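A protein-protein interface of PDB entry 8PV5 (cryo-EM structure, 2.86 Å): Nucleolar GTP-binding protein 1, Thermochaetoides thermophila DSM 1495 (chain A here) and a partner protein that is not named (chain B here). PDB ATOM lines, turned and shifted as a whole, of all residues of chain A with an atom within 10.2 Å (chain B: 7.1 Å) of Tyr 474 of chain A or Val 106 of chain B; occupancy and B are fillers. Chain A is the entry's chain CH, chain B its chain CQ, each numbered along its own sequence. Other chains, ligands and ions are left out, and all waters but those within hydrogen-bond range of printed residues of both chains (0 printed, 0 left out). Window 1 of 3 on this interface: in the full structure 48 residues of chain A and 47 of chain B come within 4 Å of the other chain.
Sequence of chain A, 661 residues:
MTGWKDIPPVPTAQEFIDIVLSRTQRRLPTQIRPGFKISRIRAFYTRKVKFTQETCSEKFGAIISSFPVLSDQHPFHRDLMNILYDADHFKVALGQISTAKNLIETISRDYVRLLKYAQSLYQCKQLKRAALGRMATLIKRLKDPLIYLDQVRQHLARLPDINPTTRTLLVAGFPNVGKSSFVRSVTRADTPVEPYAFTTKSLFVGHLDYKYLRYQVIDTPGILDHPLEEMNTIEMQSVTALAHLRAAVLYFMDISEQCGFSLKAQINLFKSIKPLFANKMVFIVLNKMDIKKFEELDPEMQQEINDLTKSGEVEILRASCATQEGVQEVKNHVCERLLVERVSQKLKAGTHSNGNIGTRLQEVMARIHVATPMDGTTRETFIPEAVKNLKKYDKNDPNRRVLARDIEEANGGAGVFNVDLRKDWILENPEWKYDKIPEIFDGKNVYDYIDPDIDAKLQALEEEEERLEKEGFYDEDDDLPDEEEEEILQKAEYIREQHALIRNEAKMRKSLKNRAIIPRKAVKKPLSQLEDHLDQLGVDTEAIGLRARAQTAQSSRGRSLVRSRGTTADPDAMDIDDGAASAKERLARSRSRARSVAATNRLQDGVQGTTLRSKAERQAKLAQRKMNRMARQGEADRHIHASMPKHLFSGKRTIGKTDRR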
ATOM      1  N   LEU A 461     -23.829 -34.325  -1.367  1.00  0.00           N
ATOM      2  CA  LEU A 461     -22.749 -33.343  -1.418  1.00  0.00           C
ATOM      3  C   LEU A 461     -22.514 -32.705  -0.057  1.00  0.00           C
ATOM      4  O   LEU A 461     -21.365 -32.514   0.356  1.00  0.00           O
ATOM      5  CB  LEU A 461     -23.069 -32.275  -2.463  1.00  0.00           C
ATOM      6  CG  LEU A 461     -22.104 -31.095  -2.610  1.00  0.00           C
ATOM      7  CD1 LEU A 461     -20.710 -31.564  -2.988  1.00  0.00           C
ATOM      8  CD2 LEU A 461     -22.631 -30.103  -3.631  1.00  0.00           C
ATOM      9  N   GLU A 462     -23.594 -32.391   0.664  1.00  0.00           N
ATOM     10  CA  GLU A 462     -23.452 -31.908   2.034  1.00  0.00           C
ATOM     11  C   GLU A 462     -22.843 -32.973   2.940  1.00  0.00           C
ATOM     12  O   GLU A 462     -22.115 -32.644   3.886  1.00  0.00           O
ATOM     13  CB  GLU A 462     -24.803 -31.445   2.577  1.00  0.00           C
ATOM     14  CG  GLU A 462     -25.405 -30.254   1.839  1.00  0.00           C
ATOM     15  CD  GLU A 462     -24.778 -28.926   2.230  1.00  0.00           C
ATOM     16  OE1 GLU A 462     -23.965 -28.894   3.178  1.00  0.00           O
ATOM     17  OE2 GLU A 462     -25.101 -27.905   1.586  1.00  0.00           O
ATOM     18  N   GLU A 463     -23.111 -34.255   2.657  1.00  0.00           N
ATOM     19  CA  GLU A 463     -22.514 -35.322   3.460  1.00  0.00           C
ATOM     20  C   GLU A 463     -20.998 -35.381   3.287  1.00  0.00           C
ATOM     21  O   GLU A 463     -20.262 -35.443   4.280  1.00  0.00           O
ATOM     22  CB  GLU A 463     -23.152 -36.674   3.134  1.00  0.00           C
ATOM     23  CG  GLU A 463     -24.572 -36.833   3.647  1.00  0.00           C
ATOM     24  CD  GLU A 463     -25.279 -38.029   3.045  1.00  0.00           C
ATOM     25  OE1 GLU A 463     -24.633 -38.786   2.291  1.00  0.00           O
ATOM     26  OE2 GLU A 463     -26.483 -38.209   3.322  1.00  0.00           O
ATOM     27  N   GLU A 464     -20.492 -35.349   2.044  1.00  0.00           N
ATOM     28  CA  GLU A 464     -19.026 -35.350   1.944  1.00  0.00           C
ATOM     29  C   GLU A 464     -18.438 -34.000   2.340  1.00  0.00           C
ATOM     30  O   GLU A 464     -17.272 -33.931   2.741  1.00  0.00           O
ATOM     31  CB  GLU A 464     -18.434 -35.773   0.582  1.00  0.00           C
ATOM     32  CG  GLU A 464     -18.606 -34.877  -0.637  1.00  0.00           C
ATOM     33  CD  GLU A 464     -19.745 -35.291  -1.523  1.00  0.00           C
ATOM     34  OE1 GLU A 464     -20.526 -36.149  -1.103  1.00  0.00           O
ATOM     35  OE2 GLU A 464     -19.856 -34.758  -2.647  1.00  0.00           O
ATOM     36  N   GLU A 465     -19.226 -32.922   2.285  1.00  0.00           N
ATOM     37  CA  GLU A 465     -18.736 -31.637   2.781  1.00  0.00           C
ATOM     38  C   GLU A 465     -18.501 -31.677   4.289  1.00  0.00           C
ATOM     39  O   GLU A 465     -17.444 -31.249   4.776  1.00  0.00           O
ATOM     40  CB  GLU A 465     -19.713 -30.519   2.417  1.00  0.00           C
ATOM     41  CG  GLU A 465     -19.209 -29.117   2.746  1.00  0.00           C
ATOM     42  CD  GLU A 465     -18.182 -28.592   1.756  1.00  0.00           C
ATOM     43  OE1 GLU A 465     -17.939 -29.249   0.721  1.00  0.00           O
ATOM     44  OE2 GLU A 465     -17.613 -27.511   2.017  1.00  0.00           O
ATOM     45  N   GLU A 466     -19.464 -32.210   5.044  1.00  0.00           N
ATOM     46  CA  GLU A 466     -19.278 -32.306   6.490  1.00  0.00           C
ATOM     47  C   GLU A 466     -18.236 -33.366   6.835  1.00  0.00           C
ATOM     48  O   GLU A 466     -17.521 -33.239   7.835  1.00  0.00           O
ATOM     49  CB  GLU A 466     -20.615 -32.572   7.195  1.00  0.00           C
ATOM     50  CG  GLU A 466     -21.343 -33.862   6.837  1.00  0.00           C
ATOM     51  CD  GLU A 466     -20.886 -35.059   7.652  1.00  0.00           C
ATOM     52  OE1 GLU A 466     -20.291 -34.853   8.732  1.00  0.00           O
ATOM     53  OE2 GLU A 466     -21.117 -36.205   7.212  1.00  0.00           O
ATOM     54  N   ARG A 467     -18.113 -34.403   5.999  1.00  0.00           N
ATOM     55  CA  ARG A 467     -17.060 -35.397   6.203  1.00  0.00           C
ATOM     56  C   ARG A 467     -15.674 -34.780   6.036  1.00  0.00           C
ATOM     57  O   ARG A 467     -14.765 -35.043   6.831  1.00  0.00           O
ATOM     58  CB  ARG A 467     -17.247 -36.565   5.234  1.00  0.00           C
ATOM     59  CG  ARG A 467     -16.261 -37.699   5.447  1.00  0.00           C
ATOM     60  CD  ARG A 467     -16.500 -38.836   4.470  1.00  0.00           C
ATOM     61  NE  ARG A 467     -16.207 -38.448   3.097  1.00  0.00           N
ATOM     62  CZ  ARG A 467     -16.491 -39.188   2.033  1.00  0.00           C
ATOM     63  NH1 ARG A 467     -17.072 -40.371   2.150  1.00  0.00           N
ATOM     64  NH2 ARG A 467     -16.183 -38.730   0.823  1.00  0.00           N
ATOM     65  N   LEU A 468     -15.498 -33.941   5.012  1.00  0.00           N
ATOM     66  CA  LEU A 468     -14.205 -33.297   4.797  1.00  0.00           C
ATOM     67  C   LEU A 468     -13.919 -32.252   5.869  1.00  0.00           C
ATOM     68  O   LEU A 468     -12.765 -32.079   6.282  1.00  0.00           O
ATOM     69  CB  LEU A 468     -14.153 -32.673   3.403  1.00  0.00           C
ATOM     70  CG  LEU A 468     -14.065 -33.648   2.227  1.00  0.00           C
ATOM     71  CD1 LEU A 468     -14.121 -32.901   0.904  1.00  0.00           C
ATOM     72  CD2 LEU A 468     -12.812 -34.505   2.315  1.00  0.00           C
ATOM     73  N   GLU A 469     -14.956 -31.546   6.335  1.00  0.00           N
ATOM     74  CA  GLU A 469     -14.762 -30.604   7.434  1.00  0.00           C
ATOM     75  C   GLU A 469     -14.393 -31.326   8.725  1.00  0.00           C
ATOM     76  O   GLU A 469     -13.623 -30.803   9.539  1.00  0.00           O
ATOM     77  CB  GLU A 469     -16.015 -29.753   7.638  1.00  0.00           C
ATOM     78  CG  GLU A 469     -16.203 -28.655   6.606  1.00  0.00           C
ATOM     79  CD  GLU A 469     -17.559 -27.986   6.713  1.00  0.00           C
ATOM     80  OE1 GLU A 469     -18.437 -28.531   7.415  1.00  0.00           O
ATOM     81  OE2 GLU A 469     -17.747 -26.914   6.101  1.00  0.00           O
ATOM     82  N   LYS A 470     -14.940 -32.527   8.934  1.00  0.00           N
ATOM     83  CA  LYS A 470     -14.540 -33.339  10.078  1.00  0.00           C
ATOM     84  C   LYS A 470     -13.100 -33.820   9.942  1.00  0.00           C
ATOM     85  O   LYS A 470     -12.330 -33.773  10.908  1.00  0.00           O
ATOM     86  CB  LYS A 470     -15.483 -34.531  10.227  1.00  0.00           C
ATOM     87  CG  LYS A 470     -15.231 -35.370  11.465  1.00  0.00           C
ATOM     88  CD  LYS A 470     -16.158 -36.570  11.507  1.00  0.00           C
ATOM     89  CE  LYS A 470     -17.578 -36.162  11.854  1.00  0.00           C
ATOM     90  NZ  LYS A 470     -18.463 -37.348  12.009  1.00  0.00           N
ATOM     91  N   GLU A 471     -12.718 -34.283   8.751  1.00  0.00           N
ATOM     92  CA  GLU A 471     -11.373 -34.801   8.528  1.00  0.00           C
ATOM     93  C   GLU A 471     -10.315 -33.711   8.427  1.00  0.00           C
ATOM     94  O   GLU A 471      -9.123 -34.037   8.430  1.00  0.00           O
ATOM     95  CB  GLU A 471     -11.342 -35.663   7.263  1.00  0.00           C
ATOM     96  CG  GLU A 471     -12.154 -36.946   7.353  1.00  0.00           C
ATOM     97  CD  GLU A 471     -11.582 -37.931   8.355  1.00  0.00           C
ATOM     98  OE1 GLU A 471     -10.344 -37.952   8.530  1.00  0.00           O
ATOM     99  OE2 GLU A 471     -12.367 -38.685   8.967  1.00  0.00           O
ATOM    100  N   GLY A 472     -10.700 -32.440   8.335  1.00  0.00           N
ATOM    101  CA  GLY A 472      -9.703 -31.393   8.253  1.00  0.00           C
ATOM    102  C   GLY A 472      -9.152 -31.166   6.867  1.00  0.00           C
ATOM    103  O   GLY A 472      -8.002 -30.746   6.725  1.00  0.00           O
ATOM    104  N   PHE A 473      -9.950 -31.446   5.835  1.00  0.00           N
ATOM    105  CA  PHE A 473      -9.535 -31.181   4.461  1.00  0.00           C
ATOM    106  C   PHE A 473      -9.415 -29.684   4.203  1.00  0.00           C
ATOM    107  O   PHE A 473      -8.637 -29.253   3.345  1.00  0.00           O
ATOM    108  CB  PHE A 473     -10.535 -31.828   3.502  1.00  0.00           C
ATOM    109  CG  PHE A 473     -10.274 -31.552   2.046  1.00  0.00           C
ATOM    110  CD1 PHE A 473     -10.989 -30.572   1.374  1.00  0.00           C
ATOM    111  CD2 PHE A 473      -9.336 -32.290   1.343  1.00  0.00           C
ATOM    112  CE1 PHE A 473     -10.763 -30.322   0.035  1.00  0.00           C
ATOM    113  CE2 PHE A 473      -9.104 -32.046   0.000  1.00  0.00           C
ATOM    114  CZ  PHE A 473      -9.820 -31.060  -0.653  1.00  0.00           C
ATOM    115  N   TYR A 474     -10.171 -28.877   4.940  1.00  0.00           N
ATOM    116  CA  TYR A 474     -10.233 -27.444   4.710  1.00  0.00           C
ATOM    117  C   TYR A 474      -9.399 -26.652   5.711  1.00  0.00           C
ATOM    118  O   TYR A 474      -9.482 -25.420   5.729  1.00  0.00           O
ATOM    119  CB  TYR A 474     -11.687 -26.978   4.773  1.00  0.00           C
ATOM    120  CG  TYR A 474     -12.551 -27.517   3.658  1.00  0.00           C
ATOM    121  CD1 TYR A 474     -12.543 -26.942   2.395  1.00  0.00           C
ATOM    122  CD2 TYR A 474     -13.388 -28.605   3.879  1.00  0.00           C
ATOM    123  CE1 TYR A 474     -13.345 -27.437   1.381  1.00  0.00           C
ATOM    124  CE2 TYR A 474     -14.190 -29.104   2.875  1.00  0.00           C
ATOM    125  CZ  TYR A 474     -14.164 -28.520   1.631  1.00  0.00           C
ATOM    126  OH  TYR A 474     -14.969 -29.032   0.642  1.00  0.00           O
ATOM    127  N   ASP A 475      -8.604 -27.328   6.536  1.00  0.00           N
ATOM    128  CA  ASP A 475      -7.886 -26.675   7.624  1.00  0.00           C
ATOM    129  C   ASP A 475      -6.665 -25.936   7.087  1.00  0.00           C
ATOM    130  O   ASP A 475      -5.907 -26.481   6.277  1.00  0.00           O
ATOM    131  CB  ASP A 475      -7.475 -27.705   8.674  1.00  0.00           C
ATOM    132  CG  ASP A 475      -8.643 -28.168   9.518  1.00  0.00           C
ATOM    133  OD1 ASP A 475      -9.799 -27.894   9.134  1.00  0.00           O
ATOM    134  OD2 ASP A 475      -8.406 -28.805  10.566  1.00  0.00           O
ATOM    135  N   GLU A 476      -6.475 -24.701   7.544  1.00  0.00           N
ATOM    136  CA  GLU A 476      -5.332 -23.882   7.164  1.00  0.00           C
ATOM    137  C   GLU A 476      -4.313 -23.876   8.297  1.00  0.00           C
ATOM    138  O   GLU A 476      -4.672 -24.060   9.466  1.00  0.00           O
ATOM    139  CB  GLU A 476      -5.770 -22.453   6.825  1.00  0.00           C
ATOM    140  CG  GLU A 476      -6.263 -21.622   8.009  1.00  0.00           C
ATOM    141  CD  GLU A 476      -7.736 -21.838   8.332  1.00  0.00           C
ATOM    142  OE1 GLU A 476      -8.326 -22.831   7.857  1.00  0.00           O
ATOM    143  OE2 GLU A 476      -8.304 -21.004   9.068  1.00  0.00           O
ATOM    144  N   ASP A 477      -3.044 -23.689   7.948  1.00  0.00           N
ATOM    145  CA  ASP A 477      -1.973 -23.668   8.936  1.00  0.00           C
ATOM    146  C   ASP A 477      -1.934 -22.335   9.678  1.00  0.00           C
ATOM    147  O   ASP A 477      -2.445 -21.326   9.191  1.00  0.00           O
ATOM    148  CB  ASP A 477      -0.624 -23.939   8.269  1.00  0.00           C
ATOM    149  CG  ASP A 477      -0.506 -25.358   7.750  1.00  0.00           C
ATOM    150  OD1 ASP A 477      -1.169 -26.254   8.312  1.00  0.00           O
ATOM    151  OD2 ASP A 477       0.252 -25.578   6.782  1.00  0.00           O
ATOM    152  N   MET B  63      -9.063 -27.790 -11.336  1.00  0.00           N
ATOM    153  CA  MET B  63      -9.738 -28.831 -10.572  1.00  0.00           C
ATOM    154  C   MET B  63     -10.835 -29.460 -11.422  1.00  0.00           C
ATOM    155  O   MET B  63     -11.891 -28.854 -11.632  1.00  0.00           O
ATOM    156  CB  MET B  63     -10.311 -28.237  -9.289  1.00  0.00           C
ATOM    157  CG  MET B  63     -10.997 -29.227  -8.375  1.00  0.00           C
ATOM    158  SD  MET B  63     -11.602 -28.408  -6.890  1.00  0.00           S
ATOM    159  CE  MET B  63     -12.972 -27.467  -7.556  1.00  0.00           C
ATOM    160  N   ASP B  66     -13.888 -33.785  -9.265  1.00  0.00           N
ATOM    161  CA  ASP B  66     -14.605 -33.301  -8.097  1.00  0.00           C
ATOM    162  C   ASP B  66     -16.068 -33.698  -8.218  1.00  0.00           C
ATOM    163  O   ASP B  66     -16.582 -33.901  -9.321  1.00  0.00           O
ATOM    164  CB  ASP B  66     -14.481 -31.780  -7.947  1.00  0.00           C
ATOM    165  CG  ASP B  66     -14.707 -31.309  -6.523  1.00  0.00           C
ATOM    166  OD1 ASP B  66     -15.383 -32.018  -5.749  1.00  0.00           O
ATOM    167  OD2 ASP B  66     -14.209 -30.220  -6.176  1.00  0.00           O
ATOM    168  N   ILE B  99     -19.242 -24.118  -2.624  1.00  0.00           N
ATOM    169  CA  ILE B  99     -18.473 -25.344  -2.391  1.00  0.00           C
ATOM    170  C   ILE B  99     -17.364 -25.502  -3.429  1.00  0.00           C
ATOM    171  O   ILE B  99     -16.216 -25.822  -3.086  1.00  0.00           O
ATOM    172  CB  ILE B  99     -19.405 -26.571  -2.355  1.00  0.00           C
ATOM    173  CG1 ILE B  99     -20.353 -26.485  -1.158  1.00  0.00           C
ATOM    174  CG2 ILE B  99     -18.605 -27.862  -2.304  1.00  0.00           C
ATOM    175  CD1 ILE B  99     -21.366 -27.602  -1.099  1.00  0.00           C
ATOM    176  N   ARG B 100     -17.678 -25.245  -4.703  1.00  0.00           N
ATOM    177  CA  ARG B 100     -16.686 -25.353  -5.768  1.00  0.00           C
ATOM    178  C   ARG B 100     -15.554 -24.351  -5.587  1.00  0.00           C
ATOM    179  O   ARG B 100     -14.376 -24.706  -5.738  1.00  0.00           O
ATOM    180  CB  ARG B 100     -17.360 -25.155  -7.126  1.00  0.00           C
ATOM    181  CG  ARG B 100     -16.444 -25.345  -8.321  1.00  0.00           C
ATOM    182  CD  ARG B 100     -17.238 -25.568  -9.597  1.00  0.00           C
ATOM    183  NE  ARG B 100     -16.511 -25.114 -10.777  1.00  0.00           N
ATOM    184  CZ  ARG B 100     -17.044 -24.996 -11.986  1.00  0.00           C
ATOM    185  NH1 ARG B 100     -18.309 -25.303 -12.215  1.00  0.00           N
ATOM    186  NH2 ARG B 100     -16.285 -24.568 -12.991  1.00  0.00           N
ATOM    187  N   ALA B 101     -15.886 -23.098  -5.244  1.00  0.00           N
ATOM    188  CA  ALA B 101     -14.845 -22.090  -5.054  1.00  0.00           C
ATOM    189  C   ALA B 101     -13.920 -22.447  -3.894  1.00  0.00           C
ATOM    190  O   ALA B 101     -12.693 -22.302  -3.993  1.00  0.00           O
ATOM    191  CB  ALA B 101     -15.483 -20.719  -4.827  1.00  0.00           C
ATOM    192  N   ARG B 102     -14.491 -22.949  -2.799  1.00  0.00           N
ATOM    193  CA  ARG B 102     -13.703 -23.222  -1.600  1.00  0.00           C
ATOM    194  C   ARG B 102     -12.810 -24.451  -1.791  1.00  0.00           C
ATOM    195  O   ARG B 102     -11.632 -24.452  -1.395  1.00  0.00           O
ATOM    196  CB  ARG B 102     -14.685 -23.340  -0.432  1.00  0.00           C
ATOM    197  CG  ARG B 102     -14.172 -23.127   0.978  1.00  0.00           C
ATOM    198  CD  ARG B 102     -15.388 -23.232   1.910  1.00  0.00           C
ATOM    199  NE  ARG B 102     -15.586 -24.470   2.652  1.00  0.00           N
ATOM    200  CZ  ARG B 102     -14.854 -24.861   3.684  1.00  0.00           C
ATOM    201  NH1 ARG B 102     -13.822 -24.152   4.112  1.00  0.00           N
ATOM    202  NH2 ARG B 102     -15.189 -25.973   4.329  1.00  0.00           N
ATOM    203  N   ARG B 103     -13.330 -25.480  -2.475  1.00  0.00           N
ATOM    204  CA  ARG B 103     -12.494 -26.626  -2.831  1.00  0.00           C
ATOM    205  C   ARG B 103     -11.390 -26.240  -3.810  1.00  0.00           C
ATOM    206  O   ARG B 103     -10.276 -26.776  -3.735  1.00  0.00           O
ATOM    207  CB  ARG B 103     -13.346 -27.750  -3.419  1.00  0.00           C
ATOM    208  CG  ARG B 103     -14.310 -28.376  -2.440  1.00  0.00           C
ATOM    209  CD  ARG B 103     -15.046 -29.548  -3.060  1.00  0.00           C
ATOM    210  NE  ARG B 103     -15.907 -30.229  -2.102  1.00  0.00           N
ATOM    211  CZ  ARG B 103     -16.690 -31.257  -2.398  1.00  0.00           C
ATOM    212  NH1 ARG B 103     -16.747 -31.752  -3.623  1.00  0.00           N
ATOM    213  NH2 ARG B 103     -17.434 -31.802  -1.440  1.00  0.00           N
ATOM    214  N   GLU B 104     -11.677 -25.323  -4.742  1.00  0.00           N
ATOM    215  CA  GLU B 104     -10.644 -24.877  -5.675  1.00  0.00           C
ATOM    216  C   GLU B 104      -9.534 -24.124  -4.948  1.00  0.00           C
ATOM    217  O   GLU B 104      -8.353 -24.249  -5.302  1.00  0.00           O
ATOM    218  CB  GLU B 104     -11.262 -24.005  -6.769  1.00  0.00           C
ATOM    219  CG  GLU B 104     -10.272 -23.543  -7.837  1.00  0.00           C
ATOM    220  CD  GLU B 104      -9.671 -22.180  -7.549  1.00  0.00           C
ATOM    221  OE1 GLU B 104     -10.080 -21.539  -6.557  1.00  0.00           O
ATOM    222  OE2 GLU B 104      -8.763 -21.766  -8.298  1.00  0.00           O
ATOM    223  N   ARG B 105      -9.895 -23.321  -3.942  1.00  0.00           N
ATOM    224  CA  ARG B 105      -8.872 -22.646  -3.144  1.00  0.00           C
ATOM    225  C   ARG B 105      -7.990 -23.654  -2.412  1.00  0.00           C
ATOM    226  O   ARG B 105      -6.763 -23.487  -2.348  1.00  0.00           O
ATOM    227  CB  ARG B 105      -9.526 -21.683  -2.153  1.00  0.00           C
ATOM    228  CG  ARG B 105      -8.571 -21.110  -1.126  1.00  0.00           C
ATOM    229  CD  ARG B 105      -9.171 -19.920  -0.409  1.00  0.00           C
ATOM    230  NE  ARG B 105      -8.924 -18.688  -1.148  1.00  0.00           N
ATOM    231  CZ  ARG B 105      -7.931 -17.849  -0.895  1.00  0.00           C
ATOM    232  NH1 ARG B 105      -7.055 -18.085   0.066  1.00  0.00           N
ATOM    233  NH2 ARG B 105      -7.804 -16.753  -1.637  1.00  0.00           N
ATOM    234  N   VAL B 106      -8.598 -24.713  -1.870  1.00  0.00           N
ATOM    235  CA  VAL B 106      -7.812 -25.789  -1.257  1.00  0.00           C
ATOM    236  C   VAL B 106      -6.863 -26.431  -2.275  1.00  0.00           C
ATOM    237  O   VAL B 106      -5.685 -26.702  -1.980  1.00  0.00           O
ATOM    238  CB  VAL B 106      -8.765 -26.819  -0.625  1.00  0.00           C
ATOM    239  CG1 VAL B 106      -7.989 -27.982  -0.076  1.00  0.00           C
ATOM    240  CG2 VAL B 106      -9.566 -26.171   0.485  1.00  0.00           C
ATOM    241  N   PHE B 107      -7.360 -26.656  -3.493  1.00  0.00           N
ATOM    242  CA  PHE B 107      -6.543 -27.212  -4.571  1.00  0.00           C
ATOM    243  C   PHE B 107      -5.346 -26.317  -4.886  1.00  0.00           C
ATOM    244  O   PHE B 107      -4.227 -26.808  -5.088  1.00  0.00           O
ATOM    245  CB  PHE B 107      -7.431 -27.411  -5.804  1.00  0.00           C
ATOM    246  CG  PHE B 107      -6.733 -28.016  -6.987  1.00  0.00           C
ATOM    247  CD1 PHE B 107      -6.538 -29.385  -7.076  1.00  0.00           C
ATOM    248  CD2 PHE B 107      -6.317 -27.218  -8.038  1.00  0.00           C
ATOM    249  CE1 PHE B 107      -5.907 -29.942  -8.175  1.00  0.00           C
ATOM    250  CE2 PHE B 107      -5.687 -27.767  -9.141  1.00  0.00           C
ATOM    251  CZ  PHE B 107      -5.482 -29.130  -9.210  1.00  0.00           C
ATOM    252  N   TYR B 108      -5.555 -24.999  -4.889  1.00  0.00           N
ATOM    253  CA  TYR B 108      -4.460 -24.067  -5.162  1.00  0.00           C
ATOM    254  C   TYR B 108      -3.440 -24.051  -4.024  1.00  0.00           C
ATOM    255  O   TYR B 108      -2.234 -23.888  -4.262  1.00  0.00           O
ATOM    256  CB  TYR B 108      -5.019 -22.667  -5.424  1.00  0.00           C
ATOM    257  CG  TYR B 108      -4.047 -21.726  -6.101  1.00  0.00           C
ATOM    258  CD1 TYR B 108      -3.846 -21.772  -7.476  1.00  0.00           C
ATOM    259  CD2 TYR B 108      -3.353 -20.777  -5.372  1.00  0.00           C
ATOM    260  CE1 TYR B 108      -2.960 -20.910  -8.096  1.00  0.00           C
ATOM    261  CE2 TYR B 108      -2.473 -19.907  -5.983  1.00  0.00           C
ATOM    262  CZ  TYR B 108      -2.280 -19.979  -7.343  1.00  0.00           C
ATOM    263  OH  TYR B 108      -1.399 -19.114  -7.947  1.00  0.00           O
ATOM    264  N   LYS B 109      -3.910 -24.208  -2.778  1.00  0.00           N
ATOM    265  CA  LYS B 109      -2.999 -24.415  -1.646  1.00  0.00           C
ATOM    266  C   LYS B 109      -2.079 -25.612  -1.863  1.00  0.00           C
ATOM    267  O   LYS B 109      -0.855 -25.508  -1.679  1.00  0.00           O
ATOM    268  CB  LYS B 109      -3.793 -24.640  -0.353  1.00  0.00           C
ATOM    269  CG  LYS B 109      -4.735 -23.544   0.154  1.00  0.00           C
ATOM    270  CD  LYS B 109      -4.033 -22.313   0.711  1.00  0.00           C
ATOM    271  CE  LYS B 109      -3.841 -21.198  -0.294  1.00  0.00           C
ATOM    272  NZ  LYS B 109      -3.252 -20.027   0.402  1.00  0.00           N
ATOM    273  N   LYS B 110      -2.655 -26.759  -2.232  1.00  0.00           N
ATOM    274  CA  LYS B 110      -1.833 -27.947  -2.470  1.00  0.00           C
ATOM    275  C   LYS B 110      -0.929 -27.792  -3.688  1.00  0.00           C
ATOM    276  O   LYS B 110       0.119 -28.443  -3.767  1.00  0.00           O
ATOM    277  CB  LYS B 110      -2.693 -29.212  -2.571  1.00  0.00           C
ATOM    278  CG  LYS B 110      -3.098 -29.803  -1.221  1.00  0.00           C
ATOM    279  CD  LYS B 110      -4.144 -29.044  -0.445  1.00  0.00           C
ATOM    280  CE  LYS B 110      -4.500 -29.803   0.824  1.00  0.00           C
ATOM    281  NZ  LYS B 110      -5.437 -29.042   1.695  1.00  0.00           N
ATOM    282  N   ARG B 111      -1.303 -26.949  -4.652  1.00  0.00           N
ATOM    283  CA  ARG B 111      -0.370 -26.697  -5.750  1.00  0.00           C
ATOM    284  C   ARG B 111       0.797 -25.809  -5.327  1.00  0.00           C
ATOM    285  O   ARG B 111       1.926 -26.022  -5.782  1.00  0.00           O
ATOM    286  CB  ARG B 111      -1.079 -26.080  -6.953  1.00  0.00           C
ATOM    287  CG  ARG B 111      -2.118 -26.976  -7.588  1.00  0.00           C
ATOM    288  CD  ARG B 111      -2.198 -26.769  -9.096  1.00  0.00           C
ATOM    289  NE  ARG B 111      -2.541 -25.400  -9.463  1.00  0.00           N
ATOM    290  CZ  ARG B 111      -1.724 -24.563 -10.088  1.00  0.00           C
ATOM    291  NH1 ARG B 111      -0.504 -24.925 -10.448  1.00  0.00           N
ATOM    292  NH2 ARG B 111      -2.147 -23.335 -10.370  1.00  0.00           N
ATOM    293  N   MET B 112       0.555 -24.814  -4.467  1.00  0.00           N
ATOM    294  CA  MET B 112       1.571 -23.823  -4.117  1.00  0.00           C
ATOM    295  C   MET B 112       2.154 -24.024  -2.719  1.00  0.00           C
ATOM    296  O   MET B 112       2.600 -23.053  -2.097  1.00  0.00           O
ATOM    297  CB  MET B 112       0.999 -22.414  -4.240  1.00  0.00           C
ATOM    298  CG  MET B 112       0.278 -22.146  -5.539  1.00  0.00           C
ATOM    299  SD  MET B 112       1.386 -21.673  -6.876  1.00  0.00           S
ATOM    300  CE  MET B 112       0.683 -22.612  -8.224  1.00  0.00           C
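The guanidinium group (NH2) of Arg 102 of chain B is in salt-bridge range of the side-chain carboxylate (OE2) of Glu 465 of chain A (3.7 Å).
NH2 of Arg 102 of chain B lies within salt-bridge range of OE2 of Glu 469 of chain A.
OE1 of Glu 465 of chain A is in salt-bridge range of NH2 of Arg 103 of chain B (3.4 Å).
NE of Arg 103 of chain B is in hydrogen-bond range of OH of Tyr 474 of chain A, at 3.1 Å.
The guanidinium group (NH1) of Arg 103 of chain B lies within salt-bridge range of the side-chain carboxylate (OD1) of Asp 66 of chain B (2.5 Å).
OE1 of Glu 465 of chain A lies within hydrogen-bond range of OH of Tyr 474 of chain A, 3.0 Å away.
The backbone NH (N) of Phe 473 of chain A sits at hydrogen-bond distance from the backbone carbonyl oxygen (O) of Leu 468 of chain A (2.9 Å).
Among the printed residues, merely in contact across the chains: Leu 461 of chain A with Ile 99 of chain B, Leu 461 of chain A with Arg 103 of chain B, Glu 464 of chain A with Arg 103 of chain B, Glu 465 of chain A with Ile 99 of chain B, Phe 473 of chain A with Val 106 of chain B, Phe 473 of chain A with Lys 110 of chain B, Tyr 474 of chain A with Arg 102 of chain B and Tyr 474 of chain A with Val 106 of chain B.
Of the printed residues of chain B, Tyr 474 of chain A touches Arg 102, Arg 103 and Val 106.
Val 106 of chain B touches just these residues of chain A: Phe 473 and Tyr 474.
Printed residues of chain A within 4 Å of Arg 102 of chain B: Glu 465, Glu 469 and Tyr 474.
Of the printed residues of chain A, Ile 99 of chain B touches Leu 461 and Glu 465.
The nearest residue of chain B that does not touch Tyr 474 of chain A is Ile 99 of chain B (4.8 Å).
The nearest printed residue of chain B that does not touch Glu 469 of chain A is Ile 99 of chain B (7.7 Å).
Of the 16 printed residues of chain B, 5 touch a printed residue of chain A.
Hydrophobic or aromatic side chains of chain B that line the printed part of chain A: Ile 99 and Val 106.
Hydrophobic or aromatic side chains of chain A that line the printed part of chain B: Leu 461, Phe 473 and Tyr 474.
Among the printed residues, 12 pairs touch across the chains.
Among the printed residues, Asp or Glu carboxylates within 4 Å of a Lys or Arg side-chain nitrogen of the other chain: Glu 465 of chain A with Arg 102 of chain B, Glu 465 of chain A with Arg 103 of chain B and Glu 469 of chain A with Arg 102 of chain B.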
